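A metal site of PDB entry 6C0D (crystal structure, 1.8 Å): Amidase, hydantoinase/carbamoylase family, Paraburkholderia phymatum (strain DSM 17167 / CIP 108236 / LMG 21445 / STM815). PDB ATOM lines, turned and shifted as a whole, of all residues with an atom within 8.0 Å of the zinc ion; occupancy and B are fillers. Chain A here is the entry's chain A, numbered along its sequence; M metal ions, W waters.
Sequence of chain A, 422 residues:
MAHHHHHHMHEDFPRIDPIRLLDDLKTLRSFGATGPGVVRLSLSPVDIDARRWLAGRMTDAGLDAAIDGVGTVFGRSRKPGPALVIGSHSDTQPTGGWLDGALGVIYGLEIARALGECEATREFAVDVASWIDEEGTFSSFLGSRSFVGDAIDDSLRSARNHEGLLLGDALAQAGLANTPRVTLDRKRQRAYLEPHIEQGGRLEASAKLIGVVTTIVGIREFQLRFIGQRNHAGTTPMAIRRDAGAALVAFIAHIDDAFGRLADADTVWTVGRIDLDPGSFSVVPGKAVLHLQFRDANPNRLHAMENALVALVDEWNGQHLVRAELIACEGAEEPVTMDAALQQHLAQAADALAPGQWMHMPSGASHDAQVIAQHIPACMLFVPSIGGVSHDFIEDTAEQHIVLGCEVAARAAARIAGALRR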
ATOM      1  N   SER A  88      27.501   2.829  12.690  1.00  0.00           N
ATOM      2  CA  SER A  88      27.625   4.274  12.707  1.00  0.00           C
ATOM      3  C   SER A  88      26.204   4.821  12.755  1.00  0.00           C
ATOM      4  O   SER A  88      25.361   4.219  13.433  1.00  0.00           O
ATOM      5  CB  SER A  88      28.388   4.784  11.476  1.00  0.00           C
ATOM      6  OG  SER A  88      28.724   6.153  11.629  1.00  0.00           O
ATOM      7  N   HIS A  89      25.919   5.920  12.058  1.00  0.00           N
ATOM      8  CA  HIS A  89      24.578   6.482  12.005  1.00  0.00           C
ATOM      9  C   HIS A  89      24.161   6.669  10.557  1.00  0.00           C
ATOM     10  O   HIS A  89      25.000   6.803   9.675  1.00  0.00           O
ATOM     11  CB  HIS A  89      24.511   7.836  12.742  1.00  0.00           C
ATOM     12  CG  HIS A  89      25.439   8.866  12.166  1.00  0.00           C
ATOM     13  ND1 HIS A  89      25.008   9.865  11.317  1.00  0.00           N
ATOM     14  CD2 HIS A  89      26.774   9.022  12.288  1.00  0.00           C
ATOM     15  CE1 HIS A  89      26.040  10.607  10.959  1.00  0.00           C
ATOM     16  NE2 HIS A  89      27.122  10.121  11.532  1.00  0.00           N
ATOM     17  N   SER A  90      22.853   6.690  10.291  1.00  0.00           N
ATOM     18  CA  SER A  90      22.404   6.971   8.928  1.00  0.00           C
ATOM     19  C   SER A  90      21.500   8.189   8.829  1.00  0.00           C
ATOM     20  O   SER A  90      20.992   8.465   7.736  1.00  0.00           O
ATOM     21  CB  SER A  90      21.695   5.729   8.345  1.00  0.00           C
ATOM     22  OG  SER A  90      20.583   5.358   9.134  1.00  0.00           O
ATOM     23  N   ASP A  91      21.295   8.921   9.923  1.00  0.00           N
ATOM     24  CA  ASP A  91      20.623  10.213   9.858  1.00  0.00           C
ATOM     25  C   ASP A  91      21.619  11.292   9.460  1.00  0.00           C
ATOM     26  O   ASP A  91      22.829  11.141   9.621  1.00  0.00           O
ATOM     27  CB  ASP A  91      19.966  10.580  11.200  1.00  0.00           C
ATOM     28  CG  ASP A  91      20.991  10.834  12.316  1.00  0.00           C
ATOM     29  OD1 ASP A  91      21.794   9.931  12.633  1.00  0.00           O
ATOM     30  OD2 ASP A  91      20.990  11.938  12.888  1.00  0.00           O
ATOM     31  N   LEU A  99      28.173  10.034   2.530  1.00  0.00           N
ATOM     32  CA  LEU A  99      29.002   9.064   3.221  1.00  0.00           C
ATOM     33  C   LEU A  99      29.137   9.304   4.719  1.00  0.00           C
ATOM     34  O   LEU A  99      29.537   8.381   5.433  1.00  0.00           O
ATOM     35  CB  LEU A  99      30.400   9.015   2.597  1.00  0.00           C
ATOM     36  CG  LEU A  99      30.429   8.631   1.107  1.00  0.00           C
ATOM     37  CD1 LEU A  99      31.821   8.828   0.530  1.00  0.00           C
ATOM     38  CD2 LEU A  99      29.970   7.192   0.924  1.00  0.00           C
ATOM     39  N   ASP A 100      28.840  10.500   5.216  1.00  0.00           N
ATOM     40  CA  ASP A 100      28.912  10.729   6.661  1.00  0.00           C
ATOM     41  C   ASP A 100      27.895   9.839   7.347  1.00  0.00           C
ATOM     42  O   ASP A 100      26.688   9.980   7.143  1.00  0.00           O
ATOM     43  CB  ASP A 100      28.665  12.199   7.012  1.00  0.00           C
ATOM     44  CG  ASP A 100      28.936  12.504   8.488  1.00  0.00           C
ATOM     45  OD1 ASP A 100      28.663  11.644   9.360  1.00  0.00           O
ATOM     46  OD2 ASP A 100      29.459  13.604   8.787  1.00  0.00           O
ATOM     47  N   GLY A 101      28.397   8.927   8.180  1.00  0.00           N
ATOM     48  CA  GLY A 101      27.549   7.978   8.848  1.00  0.00           C
ATOM     49  C   GLY A 101      27.246   6.751   8.014  1.00  0.00           C
ATOM     50  O   GLY A 101      27.504   5.626   8.444  1.00  0.00           O
ATOM     51  N   ALA A 102      26.712   6.959   6.797  1.00  0.00           N
ATOM     52  CA  ALA A 102      26.366   5.837   5.918  1.00  0.00           C
ATOM     53  C   ALA A 102      27.548   4.899   5.700  1.00  0.00           C
ATOM     54  O   ALA A 102      27.382   3.676   5.659  1.00  0.00           O
ATOM     55  CB  ALA A 102      25.872   6.379   4.571  1.00  0.00           C
ATOM     56  N   GLU A 134      22.377  10.552  15.722  1.00  0.00           N
ATOM     57  CA  GLU A 134      23.710  11.036  16.061  1.00  0.00           C
ATOM     58  C   GLU A 134      23.809  12.542  15.835  1.00  0.00           C
ATOM     59  O   GLU A 134      24.484  13.239  16.598  1.00  0.00           O
ATOM     60  CB  GLU A 134      24.760  10.301  15.228  1.00  0.00           C
ATOM     61  CG  GLU A 134      26.203  10.607  15.581  1.00  0.00           C
ATOM     62  CD  GLU A 134      26.724  11.869  14.913  1.00  0.00           C
ATOM     63  OE1 GLU A 134      26.104  12.338  13.927  1.00  0.00           O
ATOM     64  OE2 GLU A 134      27.749  12.399  15.400  1.00  0.00           O
ATOM     65  N   GLU A 135      23.129  13.062  14.815  1.00  0.00           N
ATOM     66  CA  GLU A 135      23.225  14.478  14.464  1.00  0.00           C
ATOM     67  C   GLU A 135      22.363  15.376  15.325  1.00  0.00           C
ATOM     68  O   GLU A 135      22.484  16.604  15.228  1.00  0.00           O
ATOM     69  CB  GLU A 135      22.861  14.671  12.978  1.00  0.00           C
ATOM     70  CG  GLU A 135      23.709  13.821  12.026  1.00  0.00           C
ATOM     71  CD  GLU A 135      25.083  14.420  11.751  1.00  0.00           C
ATOM     72  OE1 GLU A 135      25.456  15.405  12.428  1.00  0.00           O
ATOM     73  OE2 GLU A 135      25.779  13.914  10.834  1.00  0.00           O
ATOM     74  N   PHE A 141      23.065  11.964  19.915  1.00  0.00           N
ATOM     75  CA  PHE A 141      23.521  10.619  20.331  1.00  0.00           C
ATOM     76  C   PHE A 141      22.414   9.831  21.038  1.00  0.00           C
ATOM     77  O   PHE A 141      22.703   8.951  21.863  1.00  0.00           O
ATOM     78  CB  PHE A 141      24.765  10.683  21.223  1.00  0.00           C
ATOM     79  CG  PHE A 141      25.883  11.524  20.651  1.00  0.00           C
ATOM     80  CD1 PHE A 141      26.615  11.080  19.561  1.00  0.00           C
ATOM     81  CD2 PHE A 141      26.221  12.744  21.228  1.00  0.00           C
ATOM     82  CE1 PHE A 141      27.650  11.851  19.040  1.00  0.00           C
ATOM     83  CE2 PHE A 141      27.247  13.518  20.708  1.00  0.00           C
ATOM     84  CZ  PHE A 141      27.966  13.070  19.613  1.00  0.00           C
ATOM     85  N   GLU A 194      33.732   1.620  14.627  1.00  0.00           N
ATOM     86  CA  GLU A 194      32.991   2.606  13.813  1.00  0.00           C
ATOM     87  C   GLU A 194      33.874   3.151  12.696  1.00  0.00           C
ATOM     88  O   GLU A 194      34.695   4.056  12.926  1.00  0.00           O
ATOM     89  CB  GLU A 194      32.463   3.757  14.676  1.00  0.00           C
ATOM     90  CG  GLU A 194      31.657   4.756  13.812  1.00  0.00           C
ATOM     91  CD  GLU A 194      30.751   5.671  14.605  1.00  0.00           C
ATOM     92  OE1 GLU A 194      30.673   5.534  15.847  1.00  0.00           O
ATOM     93  OE2 GLU A 194      30.107   6.546  13.971  1.00  0.00           O
ATOM     94  N   PRO A 195      33.711   2.688  11.456  1.00  0.00           N
ATOM     95  CA  PRO A 195      34.372   3.364  10.326  1.00  0.00           C
ATOM     96  C   PRO A 195      33.667   4.687  10.045  1.00  0.00           C
ATOM     97  O   PRO A 195      32.457   4.801  10.214  1.00  0.00           O
ATOM     98  CB  PRO A 195      34.187   2.392   9.158  1.00  0.00           C
ATOM     99  CG  PRO A 195      33.661   1.065   9.792  1.00  0.00           C
ATOM    100  CD  PRO A 195      32.893   1.551  11.005  1.00  0.00           C
ATOM    101  N   HIS A 196      34.428   5.685   9.607  1.00  0.00           N
ATOM    102  CA  HIS A 196      33.821   6.988   9.314  1.00  0.00           C
ATOM    103  C   HIS A 196      34.700   7.735   8.301  1.00  0.00           C
ATOM    104  O   HIS A 196      35.917   7.539   8.272  1.00  0.00           O
ATOM    105  CB  HIS A 196      33.686   7.796  10.618  1.00  0.00           C
ATOM    106  CG  HIS A 196      32.631   8.866  10.591  1.00  0.00           C
ATOM    107  ND1 HIS A 196      32.802  10.065   9.941  1.00  0.00           N
ATOM    108  CD2 HIS A 196      31.413   8.923  11.172  1.00  0.00           C
ATOM    109  CE1 HIS A 196      31.729  10.813  10.104  1.00  0.00           C
ATOM    110  NE2 HIS A 196      30.866  10.138  10.838  1.00  0.00           N
ATOM    111  N   ILE A 197      34.088   8.629   7.501  1.00  0.00           N
ATOM    112  CA  ILE A 197      34.888   9.493   6.657  1.00  0.00           C
ATOM    113  C   ILE A 197      35.521  10.591   7.509  1.00  0.00           C
ATOM    114  O   ILE A 197      35.065  10.902   8.619  1.00  0.00           O
ATOM    115  CB  ILE A 197      34.034  10.127   5.532  1.00  0.00           C
ATOM    116  CG1 ILE A 197      32.931  10.986   6.160  1.00  0.00           C
ATOM    117  CG2 ILE A 197      33.474   9.075   4.611  1.00  0.00           C
ATOM    118  CD1 ILE A 197      32.364  12.050   5.215  1.00  0.00           C
ATOM    119  N   ALA A 365      36.276  15.485  15.558  1.00  0.00           N
ATOM    120  CA  ALA A 365      34.819  15.588  15.636  1.00  0.00           C
ATOM    121  C   ALA A 365      34.267  14.522  16.570  1.00  0.00           C
ATOM    122  O   ALA A 365      34.912  13.518  16.832  1.00  0.00           O
ATOM    123  CB  ALA A 365      34.186  15.411  14.247  1.00  0.00           C
ATOM    124  N   SER A 366      33.038  14.735  17.038  1.00  0.00           N
ATOM    125  CA  SER A 366      32.384  13.785  17.930  1.00  0.00           C
ATOM    126  C   SER A 366      31.647  12.714  17.118  1.00  0.00           C
ATOM    127  O   SER A 366      31.262  12.930  15.964  1.00  0.00           O
ATOM    128  CB  SER A 366      31.425  14.504  18.873  1.00  0.00           C
ATOM    129  OG  SER A 366      30.478  15.293  18.174  1.00  0.00           O
ATOM    130  N   HIS A 367      31.456  11.555  17.744  1.00  0.00           N
ATOM    131  CA  HIS A 367      30.861  10.383  17.091  1.00  0.00           C
ATOM    132  C   HIS A 367      30.195   9.531  18.158  1.00  0.00           C
ATOM    133  O   HIS A 367      30.497   9.643  19.346  1.00  0.00           O
ATOM    134  CB  HIS A 367      31.906   9.505  16.380  1.00  0.00           C
ATOM    135  CG  HIS A 367      32.718  10.243  15.363  1.00  0.00           C
ATOM    136  ND1 HIS A 367      32.197  10.612  14.137  1.00  0.00           N
ATOM    137  CD2 HIS A 367      33.996  10.695  15.389  1.00  0.00           C
ATOM    138  CE1 HIS A 367      33.119  11.261  13.454  1.00  0.00           C
ATOM    139  NE2 HIS A 367      34.216  11.320  14.175  1.00  0.00           N
ATOM    140  N   ASP A 368      29.287   8.652  17.715  1.00  0.00           N
ATOM    141  CA  ASP A 368      28.699   7.670  18.630  1.00  0.00           C
ATOM    142  C   ASP A 368      29.768   6.881  19.382  1.00  0.00           C
ATOM    143  O   ASP A 368      29.542   6.472  20.525  1.00  0.00           O
ATOM    144  CB  ASP A 368      27.801   6.705  17.857  1.00  0.00           C
ATOM    145  CG  ASP A 368      26.522   7.358  17.386  1.00  0.00           C
ATOM    146  OD1 ASP A 368      25.782   7.881  18.236  1.00  0.00           O
ATOM    147  OD2 ASP A 368      26.280   7.369  16.158  1.00  0.00           O
ATOM    148  N   MET A 380      37.862   3.458  16.003  1.00  0.00           N
ATOM    149  CA  MET A 380      37.393   4.071  14.758  1.00  0.00           C
ATOM    150  C   MET A 380      38.444   3.961  13.675  1.00  0.00           C
ATOM    151  O   MET A 380      39.647   4.005  13.934  1.00  0.00           O
ATOM    152  CB  MET A 380      37.040   5.561  14.949  1.00  0.00           C
ATOM    153  CG  MET A 380      35.863   5.778  15.893  1.00  0.00           C
ATOM    154  SD  MET A 380      35.261   7.498  15.781  1.00  0.00           S
ATOM    155  CE  MET A 380      34.350   7.459  14.228  1.00  0.00           C
ATOM    156  N   GLU A 395      30.503  16.654  -0.398  1.00  0.00           N
ATOM    157  CA  GLU A 395      31.324  15.662   0.289  1.00  0.00           C
ATOM    158  C   GLU A 395      31.438  14.377  -0.529  1.00  0.00           C
ATOM    159  O   GLU A 395      30.446  13.899  -1.086  1.00  0.00           O
ATOM    160  CB  GLU A 395      30.721  15.384   1.667  1.00  0.00           C
ATOM    161  CG  GLU A 395      31.050  14.032   2.304  1.00  0.00           C
ATOM    162  CD  GLU A 395      30.078  13.686   3.437  1.00  0.00           C
ATOM    163  OE1 GLU A 395      29.384  12.648   3.329  1.00  0.00           O
ATOM    164  OE2 GLU A 395      30.004  14.459   4.418  1.00  0.00           O
HETATM  165 ZN    ZN M   1      28.975  11.012  11.404  1.00  0.00          ZN
HETATM  166  O   HOH W   1      29.631  10.384  13.475  1.00  0.00           O
HETATM  167  O   HOH W   2      28.979  13.035  12.004  1.00  0.00           O
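Gly 101 touches the zinc ion (N to ZN, 3.9 Å).
The nearest printed residue that does not touch the zinc ion is Glu 134 (4.05 Å).
The zinc ion is bound by NE2 of His 89 (2.1 Å).
The zinc ion is bound by water W2, at 2.1 Å.
A ring nitrogen (NE2) of His 196 binds the zinc ion (2.2 Å).
OD1 of Asp 100 binds the zinc ion (2.2 Å).
Water W1 is bound to the zinc ion (2.3 Å).
NE2 of His 89 lies close to OE1 of Glu 134, at 3.4 Å.
A ring nitrogen (ND1) of His 89 lies within hydrogen-bond range of the backbone carbonyl oxygen (O) of Asp 91 (3.0 Å).
The backbone carbonyl oxygen of His 89 lies within hydrogen-bond range of the backbone NH of Ala 102, at 3.4 Å.
The side-chain carboxylate (OE1) of Glu 395 is in hydrogen-bond range of the backbone NH (N) of Asp 100, 2.9 Å away.
The side-chain hydroxyl (OG) of Ser 88 lies close to the backbone carbonyl oxygen (O) of Gly 101 (3.5 Å).
Water W1 lies within hydrogen-bond range of ND1 of His 367 (2.7 Å) and OE2 of Glu 134 (3.4 Å).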
